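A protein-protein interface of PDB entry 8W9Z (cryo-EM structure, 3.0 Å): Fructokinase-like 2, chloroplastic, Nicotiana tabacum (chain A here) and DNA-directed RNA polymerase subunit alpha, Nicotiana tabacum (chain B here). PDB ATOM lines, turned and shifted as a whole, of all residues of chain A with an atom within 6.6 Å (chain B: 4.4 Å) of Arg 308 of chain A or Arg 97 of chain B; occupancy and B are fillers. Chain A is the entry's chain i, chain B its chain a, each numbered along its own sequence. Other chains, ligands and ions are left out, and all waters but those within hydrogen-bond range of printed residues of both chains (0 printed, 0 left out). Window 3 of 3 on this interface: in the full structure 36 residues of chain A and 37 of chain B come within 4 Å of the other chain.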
ATOM      1  N   HIS A 303       8.886   2.347  15.089  1.00  0.00           N
ATOM      2  CA  HIS A 303       7.637   3.043  14.810  1.00  0.00           C
ATOM      3  C   HIS A 303       7.397   3.228  13.318  1.00  0.00           C
ATOM      4  O   HIS A 303       6.241   3.375  12.905  1.00  0.00           O
ATOM      5  CB  HIS A 303       7.626   4.393  15.525  1.00  0.00           C
ATOM      6  CG  HIS A 303       7.846   4.289  17.002  1.00  0.00           C
ATOM      7  ND1 HIS A 303       6.816   4.085  17.894  1.00  0.00           N
ATOM      8  CD2 HIS A 303       8.978   4.347  17.741  1.00  0.00           C
ATOM      9  CE1 HIS A 303       7.303   4.028  19.120  1.00  0.00           C
ATOM     10  NE2 HIS A 303       8.612   4.186  19.056  1.00  0.00           N
ATOM     11  N   GLU A 304       8.454   3.216  12.504  1.00  0.00           N
ATOM     12  CA  GLU A 304       8.271   3.275  11.057  1.00  0.00           C
ATOM     13  C   GLU A 304       7.553   2.037  10.538  1.00  0.00           C
ATOM     14  O   GLU A 304       6.771   2.126   9.585  1.00  0.00           O
ATOM     15  CB  GLU A 304       9.624   3.435  10.363  1.00  0.00           C
ATOM     16  CG  GLU A 304      10.383   4.693  10.754  1.00  0.00           C
ATOM     17  CD  GLU A 304       9.745   5.957  10.209  1.00  0.00           C
ATOM     18  OE1 GLU A 304       9.003   5.866   9.207  1.00  0.00           O
ATOM     19  OE2 GLU A 304       9.984   7.040  10.782  1.00  0.00           O
ATOM     20  N   TRP A 305       7.805   0.880  11.150  1.00  0.00           N
ATOM     21  CA  TRP A 305       7.122  -0.349  10.768  1.00  0.00           C
ATOM     22  C   TRP A 305       5.736  -0.462  11.388  1.00  0.00           C
ATOM     23  O   TRP A 305       4.889  -1.186  10.853  1.00  0.00           O
ATOM     24  CB  TRP A 305       7.974  -1.558  11.164  1.00  0.00           C
ATOM     25  CG  TRP A 305       7.428  -2.877  10.716  1.00  0.00           C
ATOM     26  CD1 TRP A 305       7.266  -3.302   9.431  1.00  0.00           C
ATOM     27  CD2 TRP A 305       6.998  -3.956  11.554  1.00  0.00           C
ATOM     28  NE1 TRP A 305       6.747  -4.574   9.416  1.00  0.00           N
ATOM     29  CE2 TRP A 305       6.574  -4.999  10.706  1.00  0.00           C
ATOM     30  CE3 TRP A 305       6.923  -4.139  12.937  1.00  0.00           C
ATOM     31  CZ2 TRP A 305       6.085  -6.206  11.197  1.00  0.00           C
ATOM     32  CZ3 TRP A 305       6.436  -5.339  13.423  1.00  0.00           C
ATOM     33  CH2 TRP A 305       6.025  -6.356  12.555  1.00  0.00           C
ATOM     34  N   HIS A 306       5.486   0.238  12.496  1.00  0.00           N
ATOM     35  CA  HIS A 306       4.171   0.201  13.123  1.00  0.00           C
ATOM     36  C   HIS A 306       3.198   1.181  12.481  1.00  0.00           C
ATOM     37  O   HIS A 306       1.995   0.901  12.426  1.00  0.00           O
ATOM     38  CB  HIS A 306       4.290   0.492  14.620  1.00  0.00           C
ATOM     39  CG  HIS A 306       4.832  -0.652  15.418  1.00  0.00           C
ATOM     40  ND1 HIS A 306       6.035  -1.259  15.128  1.00  0.00           N
ATOM     41  CD2 HIS A 306       4.336  -1.300  16.498  1.00  0.00           C
ATOM     42  CE1 HIS A 306       6.256  -2.230  15.994  1.00  0.00           C
ATOM     43  NE2 HIS A 306       5.240  -2.277  16.837  1.00  0.00           N
ATOM     44  N   GLU A 307       3.687   2.323  11.995  1.00  0.00           N
ATOM     45  CA  GLU A 307       2.798   3.294  11.368  1.00  0.00           C
ATOM     46  C   GLU A 307       2.316   2.838   9.998  1.00  0.00           C
ATOM     47  O   GLU A 307       1.272   3.309   9.535  1.00  0.00           O
ATOM     48  CB  GLU A 307       3.492   4.652  11.249  1.00  0.00           C
ATOM     49  CG  GLU A 307       4.678   4.668  10.301  1.00  0.00           C
ATOM     50  CD  GLU A 307       5.294   6.046  10.166  1.00  0.00           C
ATOM     51  OE1 GLU A 307       4.909   6.949  10.936  1.00  0.00           O
ATOM     52  OE2 GLU A 307       6.163   6.227   9.287  1.00  0.00           O
ATOM     53  N   ARG A 308       3.046   1.939   9.340  1.00  0.00           N
ATOM     54  CA  ARG A 308       2.637   1.436   8.036  1.00  0.00           C
ATOM     55  C   ARG A 308       1.719   0.227   8.133  1.00  0.00           C
ATOM     56  O   ARG A 308       0.842   0.054   7.279  1.00  0.00           O
ATOM     57  CB  ARG A 308       3.865   1.080   7.195  1.00  0.00           C
ATOM     58  CG  ARG A 308       4.733   2.275   6.840  1.00  0.00           C
ATOM     59  CD  ARG A 308       5.887   1.874   5.935  1.00  0.00           C
ATOM     60  NE  ARG A 308       5.423   1.219   4.715  1.00  0.00           N
ATOM     61  CZ  ARG A 308       6.216   0.866   3.710  1.00  0.00           C
ATOM     62  NH1 ARG A 308       7.519   1.108   3.773  1.00  0.00           N
ATOM     63  NH2 ARG A 308       5.708   0.271   2.639  1.00  0.00           N
ATOM     64  N   MET A 309       1.899  -0.615   9.149  1.00  0.00           N
ATOM     65  CA  MET A 309       1.064  -1.794   9.363  1.00  0.00           C
ATOM     66  C   MET A 309       0.080  -1.593  10.507  1.00  0.00           C
ATOM     67  O   MET A 309      -0.176  -2.513  11.287  1.00  0.00           O
ATOM     68  CB  MET A 309       1.933  -3.022   9.614  1.00  0.00           C
ATOM     69  CG  MET A 309       2.725  -3.480   8.404  1.00  0.00           C
ATOM     70  SD  MET A 309       3.574  -5.045   8.685  1.00  0.00           S
ATOM     71  CE  MET A 309       4.346  -5.303   7.090  1.00  0.00           C
ATOM     72  N   LYS A 310      -0.483  -0.388  10.631  1.00  0.00           N
ATOM     73  CA  LYS A 310      -1.412  -0.102  11.718  1.00  0.00           C
ATOM     74  C   LYS A 310      -2.706  -0.897  11.607  1.00  0.00           C
ATOM     75  O   LYS A 310      -3.400  -1.070  12.615  1.00  0.00           O
ATOM     76  CB  LYS A 310      -1.725   1.394  11.759  1.00  0.00           C
ATOM     77  N   ASP A 311      -3.047  -1.383  10.414  1.00  0.00           N
ATOM     78  CA  ASP A 311      -4.272  -2.146  10.222  1.00  0.00           C
ATOM     79  C   ASP A 311      -4.098  -3.637  10.474  1.00  0.00           C
ATOM     80  O   ASP A 311      -5.100  -4.359  10.545  1.00  0.00           O
ATOM     81  CB  ASP A 311      -4.809  -1.933   8.803  1.00  0.00           C
ATOM     82  CG  ASP A 311      -3.771  -2.224   7.735  1.00  0.00           C
ATOM     83  OD1 ASP A 311      -2.602  -2.480   8.092  1.00  0.00           O
ATOM     84  OD2 ASP A 311      -4.127  -2.196   6.538  1.00  0.00           O
ATOM     85  N   ALA A 312      -2.861  -4.118  10.609  1.00  0.00           N
ATOM     86  CA  ALA A 312      -2.601  -5.537  10.788  1.00  0.00           C
ATOM     87  C   ALA A 312      -1.883  -5.874  12.086  1.00  0.00           C
ATOM     88  O   ALA A 312      -1.886  -7.042  12.487  1.00  0.00           O
ATOM     89  CB  ALA A 312      -1.779  -6.075   9.607  1.00  0.00           C
ATOM     90  N   LEU B  96       1.108  -3.814  -6.490  1.00  0.00           N
ATOM     91  CA  LEU B  96       0.239  -3.280  -5.453  1.00  0.00           C
ATOM     92  C   LEU B  96       0.821  -3.605  -4.084  1.00  0.00           C
ATOM     93  O   LEU B  96       1.740  -4.418  -3.949  1.00  0.00           O
ATOM     94  CB  LEU B  96      -1.190  -3.831  -5.572  1.00  0.00           C
ATOM     95  CG  LEU B  96      -1.941  -3.565  -6.880  1.00  0.00           C
ATOM     96  CD1 LEU B  96      -1.671  -4.655  -7.908  1.00  0.00           C
ATOM     97  CD2 LEU B  96      -3.430  -3.423  -6.627  1.00  0.00           C
ATOM     98  N   ARG B  97       0.270  -2.960  -3.059  1.00  0.00           N
ATOM     99  CA  ARG B  97       0.761  -3.094  -1.694  1.00  0.00           C
ATOM    100  C   ARG B  97      -0.420  -3.211  -0.745  1.00  0.00           C
ATOM    101  O   ARG B  97      -1.336  -2.383  -0.786  1.00  0.00           O
ATOM    102  CB  ARG B  97       1.640  -1.899  -1.312  1.00  0.00           C
ATOM    103  CG  ARG B  97       2.101  -1.888   0.133  1.00  0.00           C
ATOM    104  CD  ARG B  97       3.012  -0.701   0.397  1.00  0.00           C
ATOM    105  NE  ARG B  97       2.393   0.558  -0.008  1.00  0.00           N
ATOM    106  CZ  ARG B  97       2.998   1.740   0.045  1.00  0.00           C
ATOM    107  NH1 ARG B  97       4.244   1.831   0.487  1.00  0.00           N
ATOM    108  NH2 ARG B  97       2.356   2.832  -0.345  1.00  0.00           N
ATOM    109  N   SER B  98      -0.395  -4.232   0.107  1.00  0.00           N
ATOM    110  CA  SER B  98      -1.475  -4.470   1.056  1.00  0.00           C
ATOM    111  C   SER B  98      -0.919  -5.254   2.236  1.00  0.00           C
ATOM    112  O   SER B  98       0.198  -5.774   2.192  1.00  0.00           O
ATOM    113  CB  SER B  98      -2.642  -5.215   0.402  1.00  0.00           C
ATOM    114  OG  SER B  98      -3.677  -5.461   1.336  1.00  0.00           O
ATOM    115  N   ASN B  99      -1.722  -5.332   3.300  1.00  0.00           N
ATOM    116  CA  ASN B  99      -1.330  -6.041   4.509  1.00  0.00           C
ATOM    117  C   ASN B  99      -2.413  -6.957   5.060  1.00  0.00           C
ATOM    118  O   ASN B  99      -2.173  -7.628   6.070  1.00  0.00           O
ATOM    119  CB  ASN B  99      -0.916  -5.046   5.603  1.00  0.00           C
ATOM    120  CG  ASN B  99       0.250  -4.173   5.188  1.00  0.00           C
ATOM    121  OD1 ASN B  99       0.146  -2.947   5.168  1.00  0.00           O
ATOM    122  ND2 ASN B  99       1.370  -4.804   4.852  1.00  0.00           N
ATOM    123  N   TYR B 126      -7.434   0.064   1.857  1.00  0.00           N
ATOM    124  CA  TYR B 126      -6.343  -0.761   2.358  1.00  0.00           C
ATOM    125  C   TYR B 126      -5.225  -0.935   1.336  1.00  0.00           C
ATOM    126  O   TYR B 126      -4.045  -0.920   1.703  1.00  0.00           O
ATOM    127  CB  TYR B 126      -6.874  -2.133   2.781  1.00  0.00           C
ATOM    128  CG  TYR B 126      -8.018  -2.062   3.764  1.00  0.00           C
ATOM    129  CD1 TYR B 126      -7.792  -1.763   5.100  1.00  0.00           C
ATOM    130  CD2 TYR B 126      -9.324  -2.294   3.357  1.00  0.00           C
ATOM    131  CE1 TYR B 126      -8.835  -1.697   6.004  1.00  0.00           C
ATOM    132  CE2 TYR B 126     -10.375  -2.231   4.253  1.00  0.00           C
ATOM    133  CZ  TYR B 126     -10.124  -1.931   5.576  1.00  0.00           C
ATOM    134  OH  TYR B 126     -11.165  -1.867   6.472  1.00  0.00           O
ATOM    135  N   VAL B 127      -5.569  -1.102   0.065  1.00  0.00           N
ATOM    136  CA  VAL B 127      -4.589  -1.353  -0.986  1.00  0.00           C
ATOM    137  C   VAL B 127      -4.148  -0.027  -1.589  1.00  0.00           C
ATOM    138  O   VAL B 127      -4.954   0.895  -1.758  1.00  0.00           O
ATOM    139  CB  VAL B 127      -5.172  -2.289  -2.061  1.00  0.00           C
ATOM    140  CG1 VAL B 127      -4.104  -2.680  -3.067  1.00  0.00           C
ATOM    141  CG2 VAL B 127      -5.775  -3.523  -1.416  1.00  0.00           C
ATOM    142  N   GLU B 128      -2.861   0.070  -1.913  1.00  0.00           N
ATOM    143  CA  GLU B 128      -2.292   1.242  -2.562  1.00  0.00           C
ATOM    144  C   GLU B 128      -1.464   0.799  -3.761  1.00  0.00           C
ATOM    145  O   GLU B 128      -1.165  -0.386  -3.937  1.00  0.00           O
ATOM    146  CB  GLU B 128      -1.427   2.063  -1.594  1.00  0.00           C
ATOM    147  CG  GLU B 128      -2.179   2.647  -0.406  1.00  0.00           C
ATOM    148  CD  GLU B 128      -2.393   1.639   0.708  1.00  0.00           C
ATOM    149  OE1 GLU B 128      -1.800   0.542   0.640  1.00  0.00           O
ATOM    150  OE2 GLU B 128      -3.154   1.944   1.650  1.00  0.00           O
ATOM    151  N   VAL B 130       2.102   1.578  -6.234  1.00  0.00           N
ATOM    152  CA  VAL B 130       3.497   1.964  -6.072  1.00  0.00           C
ATOM    153  C   VAL B 130       4.016   2.708  -7.299  1.00  0.00           C
ATOM    154  O   VAL B 130       4.556   3.809  -7.187  1.00  0.00           O
ATOM    155  CB  VAL B 130       4.377   0.735  -5.759  1.00  0.00           C
ATOM    156  CG1 VAL B 130       5.823   1.156  -5.544  1.00  0.00           C
ATOM    157  CG2 VAL B 130       3.844  -0.003  -4.543  1.00  0.00           C
ATOM    158  N   SER B 208       7.187  -2.654  -3.562  1.00  0.00           N
ATOM    159  CA  SER B 208       6.098  -2.839  -2.611  1.00  0.00           C
ATOM    160  C   SER B 208       6.573  -2.697  -1.171  1.00  0.00           C
ATOM    161  O   SER B 208       5.784  -2.332  -0.294  1.00  0.00           O
ATOM    162  CB  SER B 208       5.442  -4.203  -2.823  1.00  0.00           C
ATOM    163  OG  SER B 208       6.379  -5.250  -2.658  1.00  0.00           O
ATOM    164  N   THR B 210      10.430  -1.838   1.255  1.00  0.00           N
ATOM    165  CA  THR B 210      11.848  -1.534   1.265  1.00  0.00           C
ATOM    166  C   THR B 210      12.658  -2.772   1.649  1.00  0.00           C
ATOM    167  O   THR B 210      12.137  -3.696   2.278  1.00  0.00           O
ATOM    168  CB  THR B 210      12.136  -0.394   2.237  1.00  0.00           C
ATOM    169  OG1 THR B 210      11.755  -0.785   3.562  1.00  0.00           O
ATOM    170  CG2 THR B 210      11.360   0.848   1.841  1.00  0.00           C
ATOM    171  N   GLU B 213      12.472  -3.640   5.401  1.00  0.00           N
ATOM    172  CA  GLU B 213      11.243  -4.317   5.797  1.00  0.00           C
ATOM    173  C   GLU B 213      11.238  -5.765   5.328  1.00  0.00           C
ATOM    174  O   GLU B 213      10.759  -6.651   6.044  1.00  0.00           O
ATOM    175  CB  GLU B 213      10.031  -3.567   5.246  1.00  0.00           C
ATOM    176  CG  GLU B 213       9.860  -2.172   5.817  1.00  0.00           C
ATOM    177  CD  GLU B 213       8.650  -1.457   5.254  1.00  0.00           C
ATOM    178  OE1 GLU B 213       7.934  -2.058   4.427  1.00  0.00           O
ATOM    179  OE2 GLU B 213       8.415  -0.293   5.639  1.00  0.00           O
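Arg 308 of chain A touches just these residues of chain B: Arg 97, Asn 99, Ser 208 and Glu 213.
Of the printed residues of chain B, Met 309 of chain A touches Asn 99 (3.8 Å).
Arg 97 of chain B touches just one residue of chain A: Arg 308 (3.0 Å).
Printed residues of chain A within 4 Å of Tyr 126 of chain B: Asp 311 (3.96 Å).
Of the printed residues of chain A, Ser 208 of chain B touches Arg 308.
Printed residues of chain A within 4 Å of Glu 213 of chain B: Arg 308.
The nearest printed residue of chain A that does not touch Arg 97 of chain B is Asp 311 of chain A (7.8 Å).
Of the 10 printed residues of chain A, 4 touch a printed residue of chain B.
Hydrophobic or aromatic side chains of chain B that line the printed part of chain A: Tyr 126.
Among the printed residues, 8 pairs touch across the chains.
Among the printed residues, Asp or Glu carboxylates within 4 Å of a Lys or Arg side-chain nitrogen of the other chain: Arg 308 of chain A with Glu 213 of chain B (2.5 Å).
Among the printed residues, merely in contact across the chains: Arg 308 of chain A with Asn 99 of chain B, Met 309 of chain A with Asn 99 of chain B, Ala 312 of chain A with Asn 99 of chain B, Arg 308 of chain A with Ser 208 of chain B, Asp 311 of chain A with Asn 99 of chain B and Asp 311 of chain A with Tyr 126 of chain B.
The side-chain carboxylate (OE2) of Glu 213 of chain B is in salt-bridge range of the guanidinium group (NH1) of Arg 308 of chain A (2.5 Å).
The guanidinium group (NH1) of Arg 97 of chain B sits close to the guanidinium group (NH2) of Arg 308 of chain A (3.0 Å).
The side-chain hydroxyl (OG1) of Thr 210 of chain B sits close to the backbone NH (N) of Glu 213 of chain B (3.5 Å).
The backbone NH (N) of Arg 97 of chain B is in hydrogen-bond range of the backbone carbonyl oxygen (O) of Glu 128 of chain B (3.1 Å).
The side-chain sulfur (SD) of Met 309 of chain A is in hydrogen-bond range of the indole nitrogen (NE1) of Trp 305 of chain A, 3.3 Å away.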
